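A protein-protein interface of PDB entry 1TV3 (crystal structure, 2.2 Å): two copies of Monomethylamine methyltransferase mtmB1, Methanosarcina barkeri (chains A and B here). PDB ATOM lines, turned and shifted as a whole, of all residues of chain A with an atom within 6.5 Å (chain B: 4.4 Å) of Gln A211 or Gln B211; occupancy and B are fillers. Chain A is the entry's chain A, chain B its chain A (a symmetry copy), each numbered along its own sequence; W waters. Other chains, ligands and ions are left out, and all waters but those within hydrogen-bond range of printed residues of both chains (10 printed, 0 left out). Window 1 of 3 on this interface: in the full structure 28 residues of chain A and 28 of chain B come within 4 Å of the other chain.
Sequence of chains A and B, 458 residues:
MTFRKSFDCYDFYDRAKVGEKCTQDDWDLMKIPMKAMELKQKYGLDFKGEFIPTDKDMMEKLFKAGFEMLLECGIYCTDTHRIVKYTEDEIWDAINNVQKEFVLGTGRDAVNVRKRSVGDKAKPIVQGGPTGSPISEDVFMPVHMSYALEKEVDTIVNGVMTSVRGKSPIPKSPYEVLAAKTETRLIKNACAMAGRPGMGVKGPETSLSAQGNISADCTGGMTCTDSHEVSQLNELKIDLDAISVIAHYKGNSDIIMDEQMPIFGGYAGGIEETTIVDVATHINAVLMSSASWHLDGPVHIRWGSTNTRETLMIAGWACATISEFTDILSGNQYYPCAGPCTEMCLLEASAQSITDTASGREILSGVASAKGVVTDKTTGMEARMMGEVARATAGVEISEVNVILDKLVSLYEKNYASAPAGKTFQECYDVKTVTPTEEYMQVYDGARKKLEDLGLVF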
ATOM      1  N   PRO A 171      -8.344 -25.707  -1.843  1.00  0.00           N
ATOM      2  CA  PRO A 171      -7.973 -24.887  -0.689  1.00  0.00           C
ATOM      3  C   PRO A 171      -6.803 -23.959  -0.994  1.00  0.00           C
ATOM      4  O   PRO A 171      -5.811 -24.373  -1.599  1.00  0.00           O
ATOM      5  CB  PRO A 171      -7.632 -25.929   0.371  1.00  0.00           C
ATOM      6  CG  PRO A 171      -8.596 -27.029   0.056  1.00  0.00           C
ATOM      7  CD  PRO A 171      -8.497 -27.121  -1.455  1.00  0.00           C
ATOM      8  N   LYS A 172      -6.943 -22.704  -0.577  1.00  0.00           N
ATOM      9  CA  LYS A 172      -5.933 -21.670  -0.766  1.00  0.00           C
ATOM     10  C   LYS A 172      -5.720 -21.224  -2.207  1.00  0.00           C
ATOM     11  O   LYS A 172      -4.702 -20.613  -2.535  1.00  0.00           O
ATOM     12  CB  LYS A 172      -4.605 -22.100  -0.130  1.00  0.00           C
ATOM     13  CG  LYS A 172      -4.707 -22.199   1.387  1.00  0.00           C
ATOM     14  CD  LYS A 172      -3.381 -22.496   2.064  1.00  0.00           C
ATOM     15  CE  LYS A 172      -3.595 -22.642   3.566  1.00  0.00           C
ATOM     16  NZ  LYS A 172      -2.357 -23.003   4.315  1.00  0.00           N
ATOM     17  N   SER A 173      -6.690 -21.531  -3.064  1.00  0.00           N
ATOM     18  CA  SER A 173      -6.647 -21.112  -4.461  1.00  0.00           C
ATOM     19  C   SER A 173      -7.720 -20.028  -4.557  1.00  0.00           C
ATOM     20  O   SER A 173      -8.588 -19.935  -3.688  1.00  0.00           O
ATOM     21  CB  SER A 173      -7.023 -22.264  -5.395  1.00  0.00           C
ATOM     22  OG  SER A 173      -8.429 -22.476  -5.387  1.00  0.00           O
ATOM     23  N   PRO A 174      -7.675 -19.188  -5.601  1.00  0.00           N
ATOM     24  CA  PRO A 174      -8.707 -18.150  -5.701  1.00  0.00           C
ATOM     25  C   PRO A 174     -10.112 -18.748  -5.834  1.00  0.00           C
ATOM     26  O   PRO A 174     -11.098 -18.115  -5.458  1.00  0.00           O
ATOM     27  CB  PRO A 174      -8.280 -17.350  -6.933  1.00  0.00           C
ATOM     28  CG  PRO A 174      -7.513 -18.369  -7.763  1.00  0.00           C
ATOM     29  CD  PRO A 174      -6.701 -19.075  -6.698  1.00  0.00           C
ATOM     30  N   GLU A 176     -11.337 -21.145  -4.139  1.00  0.00           N
ATOM     31  CA  GLU A 176     -11.894 -21.429  -2.823  1.00  0.00           C
ATOM     32  C   GLU A 176     -12.612 -20.179  -2.314  1.00  0.00           C
ATOM     33  O   GLU A 176     -13.691 -20.273  -1.730  1.00  0.00           O
ATOM     34  CB  GLU A 176     -10.803 -21.835  -1.827  1.00  0.00           C
ATOM     35  CG  GLU A 176     -11.358 -22.029  -0.418  1.00  0.00           C
ATOM     36  CD  GLU A 176     -10.292 -22.310   0.621  1.00  0.00           C
ATOM     37  OE1 GLU A 176      -9.218 -21.667   0.570  1.00  0.00           O
ATOM     38  OE2 GLU A 176     -10.543 -23.162   1.502  1.00  0.00           O
ATOM     39  N   VAL A 177     -12.003 -19.014  -2.533  1.00  0.00           N
ATOM     40  CA  VAL A 177     -12.598 -17.746  -2.117  1.00  0.00           C
ATOM     41  C   VAL A 177     -13.884 -17.512  -2.906  1.00  0.00           C
ATOM     42  O   VAL A 177     -14.911 -17.147  -2.335  1.00  0.00           O
ATOM     43  CB  VAL A 177     -11.622 -16.559  -2.356  1.00  0.00           C
ATOM     44  CG1 VAL A 177     -12.370 -15.228  -2.312  1.00  0.00           C
ATOM     45  CG2 VAL A 177     -10.534 -16.573  -1.294  1.00  0.00           C
ATOM     46  N   ALA A 180     -16.577 -19.730  -1.554  1.00  0.00           N
ATOM     47  CA  ALA A 180     -17.019 -19.335  -0.217  1.00  0.00           C
ATOM     48  C   ALA A 180     -18.094 -18.246  -0.275  1.00  0.00           C
ATOM     49  O   ALA A 180     -19.080 -18.292   0.464  1.00  0.00           O
ATOM     50  CB  ALA A 180     -15.826 -18.853   0.611  1.00  0.00           C
ATOM     51  N   SER A 207     -15.401 -23.914   1.575  1.00  0.00           N
ATOM     52  CA  SER A 207     -14.067 -23.465   1.957  1.00  0.00           C
ATOM     53  C   SER A 207     -13.570 -24.275   3.147  1.00  0.00           C
ATOM     54  O   SER A 207     -14.353 -24.638   4.025  1.00  0.00           O
ATOM     55  CB  SER A 207     -14.088 -21.974   2.316  1.00  0.00           C
ATOM     56  OG  SER A 207     -15.151 -21.676   3.210  1.00  0.00           O
ATOM     57  N   LEU A 208     -12.269 -24.554   3.172  1.00  0.00           N
ATOM     58  CA  LEU A 208     -11.668 -25.331   4.256  1.00  0.00           C
ATOM     59  C   LEU A 208     -10.551 -24.569   4.957  1.00  0.00           C
ATOM     60  O   LEU A 208     -10.312 -24.765   6.150  1.00  0.00           O
ATOM     61  CB  LEU A 208     -11.112 -26.656   3.714  1.00  0.00           C
ATOM     62  CG  LEU A 208     -12.111 -27.572   2.994  1.00  0.00           C
ATOM     63  CD1 LEU A 208     -11.387 -28.793   2.434  1.00  0.00           C
ATOM     64  CD2 LEU A 208     -13.204 -27.993   3.962  1.00  0.00           C
ATOM     65  N   SER A 209      -9.861 -23.708   4.219  1.00  0.00           N
ATOM     66  CA  SER A 209      -8.768 -22.938   4.797  1.00  0.00           C
ATOM     67  C   SER A 209      -9.299 -21.728   5.550  1.00  0.00           C
ATOM     68  O   SER A 209     -10.444 -21.317   5.356  1.00  0.00           O
ATOM     69  CB  SER A 209      -7.817 -22.459   3.705  1.00  0.00           C
ATOM     70  OG  SER A 209      -8.414 -21.425   2.945  1.00  0.00           O
ATOM     71  N   ALA A 210      -8.455 -21.157   6.401  1.00  0.00           N
ATOM     72  CA  ALA A 210      -8.832 -19.982   7.171  1.00  0.00           C
ATOM     73  C   ALA A 210      -9.204 -18.831   6.234  1.00  0.00           C
ATOM     74  O   ALA A 210     -10.239 -18.184   6.420  1.00  0.00           O
ATOM     75  CB  ALA A 210      -7.685 -19.565   8.086  1.00  0.00           C
ATOM     76  N   GLN A 211      -8.372 -18.580   5.224  1.00  0.00           N
ATOM     77  CA  GLN A 211      -8.644 -17.491   4.288  1.00  0.00           C
ATOM     78  C   GLN A 211      -9.941 -17.729   3.521  1.00  0.00           C
ATOM     79  O   GLN A 211     -10.690 -16.789   3.246  1.00  0.00           O
ATOM     80  CB  GLN A 211      -7.476 -17.304   3.312  1.00  0.00           C
ATOM     81  CG  GLN A 211      -7.209 -18.474   2.383  1.00  0.00           C
ATOM     82  CD  GLN A 211      -5.810 -18.420   1.799  1.00  0.00           C
ATOM     83  OE1 GLN A 211      -4.827 -18.438   2.536  1.00  0.00           O
ATOM     84  NE2 GLN A 211      -5.712 -18.351   0.472  1.00  0.00           N
ATOM     85  N   GLY A 212     -10.204 -18.987   3.178  1.00  0.00           N
ATOM     86  CA  GLY A 212     -11.425 -19.307   2.467  1.00  0.00           C
ATOM     87  C   GLY A 212     -12.639 -19.007   3.331  1.00  0.00           C
ATOM     88  O   GLY A 212     -13.552 -18.303   2.905  1.00  0.00           O
ATOM     89  N   ASN A 213     -12.647 -19.531   4.554  1.00  0.00           N
ATOM     90  CA  ASN A 213     -13.769 -19.309   5.459  1.00  0.00           C
ATOM     91  C   ASN A 213     -13.982 -17.828   5.778  1.00  0.00           C
ATOM     92  O   ASN A 213     -15.114 -17.342   5.802  1.00  0.00           O
ATOM     93  CB  ASN A 213     -13.576 -20.097   6.761  1.00  0.00           C
ATOM     94  CG  ASN A 213     -13.688 -21.604   6.557  1.00  0.00           C
ATOM     95  OD1 ASN A 213     -14.559 -22.075   5.825  1.00  0.00           O
ATOM     96  ND2 ASN A 213     -12.813 -22.366   7.218  1.00  0.00           N
ATOM     97  N   ILE A 214     -12.889 -17.112   6.012  1.00  0.00           N
ATOM     98  CA  ILE A 214     -12.961 -15.697   6.342  1.00  0.00           C
ATOM     99  C   ILE A 214     -13.529 -14.828   5.214  1.00  0.00           C
ATOM    100  O   ILE A 214     -14.079 -13.758   5.470  1.00  0.00           O
ATOM    101  CB  ILE A 214     -11.564 -15.193   6.780  1.00  0.00           C
ATOM    102  CG1 ILE A 214     -11.222 -15.828   8.133  1.00  0.00           C
ATOM    103  CG2 ILE A 214     -11.532 -13.664   6.869  1.00  0.00           C
ATOM    104  CD1 ILE A 214      -9.822 -15.534   8.633  1.00  0.00           C
ATOM    105  N   SER A 215     -13.430 -15.296   3.974  1.00  0.00           N
ATOM    106  CA  SER A 215     -13.938 -14.530   2.836  1.00  0.00           C
ATOM    107  C   SER A 215     -15.444 -14.692   2.606  1.00  0.00           C
ATOM    108  O   SER A 215     -16.030 -13.949   1.821  1.00  0.00           O
ATOM    109  CB  SER A 215     -13.213 -14.946   1.557  1.00  0.00           C
ATOM    110  OG  SER A 215     -13.693 -16.203   1.107  1.00  0.00           O
ATOM    111  N   ALA A 216     -16.065 -15.650   3.288  1.00  0.00           N
ATOM    112  CA  ALA A 216     -17.494 -15.917   3.114  1.00  0.00           C
ATOM    113  C   ALA A 216     -18.466 -14.780   3.457  1.00  0.00           C
ATOM    114  O   ALA A 216     -19.522 -14.672   2.832  1.00  0.00           O
ATOM    115  CB  ALA A 216     -17.880 -17.174   3.880  1.00  0.00           C
ATOM    116  N   LEU A 240      -4.668 -23.874  14.770  1.00  0.00           N
ATOM    117  CA  LEU A 240      -4.635 -22.417  14.817  1.00  0.00           C
ATOM    118  C   LEU A 240      -5.474 -21.724  13.745  1.00  0.00           C
ATOM    119  O   LEU A 240      -5.937 -20.605  13.954  1.00  0.00           O
ATOM    120  CB  LEU A 240      -3.186 -21.922  14.771  1.00  0.00           C
ATOM    121  CG  LEU A 240      -2.362 -22.271  16.018  1.00  0.00           C
ATOM    122  CD1 LEU A 240      -0.985 -21.638  15.914  1.00  0.00           C
ATOM    123  CD2 LEU A 240      -3.072 -21.780  17.273  1.00  0.00           C
ATOM    124  N   ASP A 241      -5.668 -22.378  12.603  1.00  0.00           N
ATOM    125  CA  ASP A 241      -6.489 -21.807  11.535  1.00  0.00           C
ATOM    126  C   ASP A 241      -7.881 -21.493  12.078  1.00  0.00           C
ATOM    127  O   ASP A 241      -8.445 -20.436  11.803  1.00  0.00           O
ATOM    128  CB  ASP A 241      -6.613 -22.796  10.373  1.00  0.00           C
ATOM    129  CG  ASP A 241      -5.657 -22.486   9.234  1.00  0.00           C
ATOM    130  OD1 ASP A 241      -4.523 -22.030   9.505  1.00  0.00           O
ATOM    131  OD2 ASP A 241      -6.039 -22.712   8.063  1.00  0.00           O
ATOM    132  N   SER A 244      -8.012 -18.334  14.254  1.00  0.00           N
ATOM    133  CA  SER A 244      -8.071 -17.078  13.509  1.00  0.00           C
ATOM    134  C   SER A 244      -9.473 -16.846  12.946  1.00  0.00           C
ATOM    135  O   SER A 244      -9.960 -15.714  12.923  1.00  0.00           O
ATOM    136  CB  SER A 244      -7.056 -17.073  12.364  1.00  0.00           C
ATOM    137  OG  SER A 244      -5.760 -16.752  12.837  1.00  0.00           O
ATOM    138  N   VAL A 245     -10.120 -17.914  12.485  1.00  0.00           N
ATOM    139  CA  VAL A 245     -11.469 -17.788  11.944  1.00  0.00           C
ATOM    140  C   VAL A 245     -12.405 -17.293  13.045  1.00  0.00           C
ATOM    141  O   VAL A 245     -13.258 -16.435  12.806  1.00  0.00           O
ATOM    142  CB  VAL A 245     -11.981 -19.131  11.386  1.00  0.00           C
ATOM    143  CG1 VAL A 245     -13.445 -19.007  10.989  1.00  0.00           C
ATOM    144  CG2 VAL A 245     -11.147 -19.534  10.174  1.00  0.00           C
ATOM    145  N   LYS B 172      -0.930 -14.839  10.619  1.00  0.00           N
ATOM    146  CA  LYS B 172      -1.675 -16.077  10.809  1.00  0.00           C
ATOM    147  C   LYS B 172      -2.061 -16.389  12.250  1.00  0.00           C
ATOM    148  O   LYS B 172      -2.396 -17.527  12.581  1.00  0.00           O
ATOM    149  CB  LYS B 172      -0.919 -17.255  10.184  1.00  0.00           C
ATOM    150  CG  LYS B 172      -0.839 -17.139   8.666  1.00  0.00           C
ATOM    151  CD  LYS B 172      -0.211 -18.350   7.999  1.00  0.00           C
ATOM    152  CE  LYS B 172      -0.114 -18.113   6.496  1.00  0.00           C
ATOM    153  NZ  LYS B 172       0.553 -19.222   5.757  1.00  0.00           N
ATOM    154  N   GLU B 176      -3.574 -10.967  14.146  1.00  0.00           N
ATOM    155  CA  GLU B 176      -3.433 -10.362  12.828  1.00  0.00           C
ATOM    156  C   GLU B 176      -4.820  -9.987  12.308  1.00  0.00           C
ATOM    157  O   GLU B 176      -4.999  -8.923  11.717  1.00  0.00           O
ATOM    158  CB  GLU B 176      -2.757 -11.320  11.841  1.00  0.00           C
ATOM    159  CG  GLU B 176      -2.701 -10.740  10.429  1.00  0.00           C
ATOM    160  CD  GLU B 176      -2.152 -11.705   9.398  1.00  0.00           C
ATOM    161  OE1 GLU B 176      -2.502 -12.907   9.452  1.00  0.00           O
ATOM    162  OE2 GLU B 176      -1.386 -11.251   8.519  1.00  0.00           O
ATOM    163  N   SER B 209      -0.669 -11.784   5.809  1.00  0.00           N
ATOM    164  CA  SER B 209      -1.132 -13.040   5.234  1.00  0.00           C
ATOM    165  C   SER B 209      -2.433 -12.836   4.473  1.00  0.00           C
ATOM    166  O   SER B 209      -3.122 -11.833   4.657  1.00  0.00           O
ATOM    167  CB  SER B 209      -1.362 -14.076   6.331  1.00  0.00           C
ATOM    168  OG  SER B 209      -2.517 -13.757   7.082  1.00  0.00           O
ATOM    169  N   ALA B 210      -2.766 -13.802   3.623  1.00  0.00           N
ATOM    170  CA  ALA B 210      -3.993 -13.739   2.846  1.00  0.00           C
ATOM    171  C   ALA B 210      -5.206 -13.667   3.775  1.00  0.00           C
ATOM    172  O   ALA B 210      -6.094 -12.830   3.580  1.00  0.00           O
ATOM    173  CB  ALA B 210      -4.100 -14.959   1.936  1.00  0.00           C
ATOM    174  N   GLN B 211      -5.245 -14.530   4.788  1.00  0.00           N
ATOM    175  CA  GLN B 211      -6.373 -14.538   5.718  1.00  0.00           C
ATOM    176  C   GLN B 211      -6.476 -13.220   6.478  1.00  0.00           C
ATOM    177  O   GLN B 211      -7.578 -12.733   6.743  1.00  0.00           O
ATOM    178  CB  GLN B 211      -6.264 -15.711   6.701  1.00  0.00           C
ATOM    179  CG  GLN B 211      -5.070 -15.668   7.637  1.00  0.00           C
ATOM    180  CD  GLN B 211      -4.771 -17.033   8.229  1.00  0.00           C
ATOM    181  OE1 GLN B 211      -4.500 -17.982   7.499  1.00  0.00           O
ATOM    182  NE2 GLN B 211      -4.822 -17.138   9.557  1.00  0.00           N
ATOM    183  N   GLY B 212      -5.328 -12.645   6.826  1.00  0.00           N
ATOM    184  CA  GLY B 212      -5.333 -11.380   7.530  1.00  0.00           C
ATOM    185  C   GLY B 212      -5.926 -10.285   6.658  1.00  0.00           C
ATOM    186  O   GLY B 212      -6.841  -9.578   7.075  1.00  0.00           O
ATOM    187  N   ASN B 213      -5.414 -10.151   5.437  1.00  0.00           N
ATOM    188  CA  ASN B 213      -5.906  -9.126   4.524  1.00  0.00           C
ATOM    189  C   ASN B 213      -7.392  -9.297   4.196  1.00  0.00           C
ATOM    190  O   ASN B 213      -8.149  -8.326   4.163  1.00  0.00           O
ATOM    191  CB  ASN B 213      -5.088  -9.120   3.226  1.00  0.00           C
ATOM    192  CG  ASN B 213      -3.660  -8.627   3.437  1.00  0.00           C
ATOM    193  OD1 ASN B 213      -3.429  -7.662   4.166  1.00  0.00           O
ATOM    194  ND2 ASN B 213      -2.696  -9.284   2.786  1.00  0.00           N
ATOM    195  N   ILE B 214      -7.806 -10.537   3.965  1.00  0.00           N
ATOM    196  CA  ILE B 214      -9.190 -10.827   3.629  1.00  0.00           C
ATOM    197  C   ILE B 214     -10.182 -10.493   4.749  1.00  0.00           C
ATOM    198  O   ILE B 214     -11.355 -10.235   4.485  1.00  0.00           O
ATOM    199  CB  ILE B 214      -9.321 -12.309   3.197  1.00  0.00           C
ATOM    200  CG1 ILE B 214      -8.611 -12.486   1.849  1.00  0.00           C
ATOM    201  CG2 ILE B 214     -10.792 -12.728   3.101  1.00  0.00           C
ATOM    202  CD1 ILE B 214      -8.537 -13.916   1.357  1.00  0.00           C
ATOM    203  N   SER B 215      -9.712 -10.464   5.991  1.00  0.00           N
ATOM    204  CA  SER B 215     -10.589 -10.162   7.123  1.00  0.00           C
ATOM    205  C   SER B 215     -10.816  -8.663   7.345  1.00  0.00           C
ATOM    206  O   SER B 215     -11.688  -8.281   8.122  1.00  0.00           O
ATOM    207  CB  SER B 215     -10.010 -10.752   8.409  1.00  0.00           C
ATOM    208  OG  SER B 215      -8.919  -9.966   8.862  1.00  0.00           O
ATOM    209  N   SER B 244      -5.335 -14.984  -4.239  1.00  0.00           N
ATOM    210  CA  SER B 244      -6.569 -15.242  -3.501  1.00  0.00           C
ATOM    211  C   SER B 244      -7.153 -13.942  -2.948  1.00  0.00           C
ATOM    212  O   SER B 244      -8.371 -13.758  -2.934  1.00  0.00           O
ATOM    213  CB  SER B 244      -6.324 -16.220  -2.350  1.00  0.00           C
ATOM    214  OG  SER B 244      -6.303 -17.556  -2.816  1.00  0.00           O
HETATM  215  O   HOH W   1      -4.395 -18.326  14.353  1.00  0.00           O
HETATM  216  O   HOH W   2      -3.779 -20.470   7.049  1.00  0.00           O
HETATM  217  O   HOH W   3      -4.469 -14.480  10.871  1.00  0.00           O
HETATM  218  O   HOH W   4      -5.601 -19.646   4.968  1.00  0.00           O
HETATM  219  O   HOH W   5      -8.186 -19.372  -0.853  1.00  0.00           O
HETATM  220  O   HOH W   6      -1.713 -20.487   5.033  1.00  0.00           O
HETATM  221  O   HOH W   7      -4.014 -19.647  10.903  1.00  0.00           O
HETATM  222  O   HOH W   8     -13.837 -11.132   4.972  1.00  0.00           O
HETATM  223  O   HOH W   9      -3.512 -16.939   5.067  1.00  0.00           O
HETATM  224  O   HOH W  10      -4.425 -18.485  -4.316  1.00  0.00           O
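The backbone carbonyl oxygen (O) of Lys A172 is in hydrogen-bond range of the side-chain hydroxyl (OG) of Ser B244 (3.5 Å). The backbone carbonyl oxygen of Ser A173 lies close to the side-chain hydroxyl of Ser B244 (3.4 Å). The side-chain hydroxyl of Ser B244 is in hydrogen-bond range of the side-chain amide nitrogen of Gln A211 (3.4 Å). The side-chain hydroxyl (OG) of Ser A244 sits at hydrogen-bond distance from the backbone carbonyl oxygen (O) of Lys B172 (3.5 Å). OG of Ser A244 sits at hydrogen-bond distance from NE2 of Gln B211 (3.4 Å).
Lys A172 touches Ser B244, and with the chains exchanged Ser A244 touches Lys B172. Gln A211 touches its own counterpart, Gln B211. Ile B214 touches its own counterpart, Ile A214. Ile A214 touches Ser B215, and with the chains exchanged Ser A215 touches Ile B214. Positions printed for both chains: 172, 176, 209, 210, 211, 212, 213, 214, 215 and 244. Of the 13 pairs that touch across the chains among the printed residues, 10 have their exchanged pair printed and touching as well.
The side-chain carboxylate (OE1) of Glu A176 is in hydrogen-bond range of the backbone NH (N) of Lys A172 (2.8 Å). The backbone NH (N) of Glu A176 is in hydrogen-bond range of the side-chain hydroxyl (OG) of Ser A173 (3.4 Å). OD2 of Asp A241 is in hydrogen-bond range of N of Ala A210 (3.3 Å). The backbone carbonyl oxygen (O) of Gly A212 lies within hydrogen-bond range of the side-chain hydroxyl (OG) of Ser A215 (2.8 Å). The side-chain carboxylate of Glu B176 sits at hydrogen-bond distance from the backbone NH of Lys B172 (2.8 Å). The backbone carbonyl oxygen (O) of Gly B212 lies within hydrogen-bond range of the side-chain hydroxyl (OG) of Ser B215 (2.8 Å).
Of the 10 printed residues of chain B, 6 touch a printed residue of chain A. Hydrophobic or aromatic side chains of chain B within 4 Å of the printed part of chain A: Ala B210 and Ile B214.
Water W2 lies within hydrogen-bond range of the side-chain amide oxygen of Gln B211 (2.6 Å) and the side-chain carboxylate of Asp A241 (3.0 Å). Water W8 lies within hydrogen-bond range of the backbone carbonyl oxygen (O) of Ile A214 (2.7 Å) and the backbone carbonyl oxygen (O) of Ile B214 (2.7 Å). Water W6 lies within hydrogen-bond range of the side-chain amino group (NZ) of Lys B172 (2.7 Å) and the side-chain amino group (NZ) of Lys A172 (2.7 Å). Water W7 lies within hydrogen-bond range of the side-chain carboxylate of Asp A241, the side-chain amide nitrogen of Gln B211 and the backbone carbonyl oxygen of Lys B172. Water W9 lies within hydrogen-bond range of OE1 of Gln B211 (2.8 Å) and OE1 of Gln A211 (3.2 Å). Water W5 lies within hydrogen-bond range of OE1 of Glu A176 (2.9 Å), O of Ser A173 (2.9 Å), NE2 of Gln A211 (3.0 Å) and OG of Ser B244 (3.3 Å).
Gln A211 touches just these residues of chain B: Ala B210 (3.6 Å), Gln B211 (3.8 Å) and Ser B244 (3.4 Å). Of chain A, only Ala A210, Gln A211 and Ser A244 come within 4 Å of Gln B211. Printed residues of chain A within 4 Å of Ser B215: Ile A214. Of the printed residues of chain B, Ser A244 touches Lys B172 and Gln B211. Of the printed residues of chain B, Val A177 touches Ser B244 (3.9 Å). Of the printed residues of chain B, Ser A215 touches Ile B214 (3.6 Å). Of the printed residues of chain B, Ser A173 touches Ser B244. Glu B176 touches none of the printed residues of chain A. Gly B212 touches none of the printed residues of chain A.
Among the printed residues, pairs that only touch across the chains: Pro A174 with Ser B244 (3.5 Å), Gln A211 with Ala B210 (3.6 Å), Ala A210 with Gln B211 (3.6 Å), Ser A215 with Ile B214 (3.6 Å), Ile A214 with Ser B215 (3.6 Å), Gln A211 with Gln B211 (3.8 Å), Val A177 with Ser B244 (3.9 Å) and Ile A214 with Ile B214 (3.95 Å).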
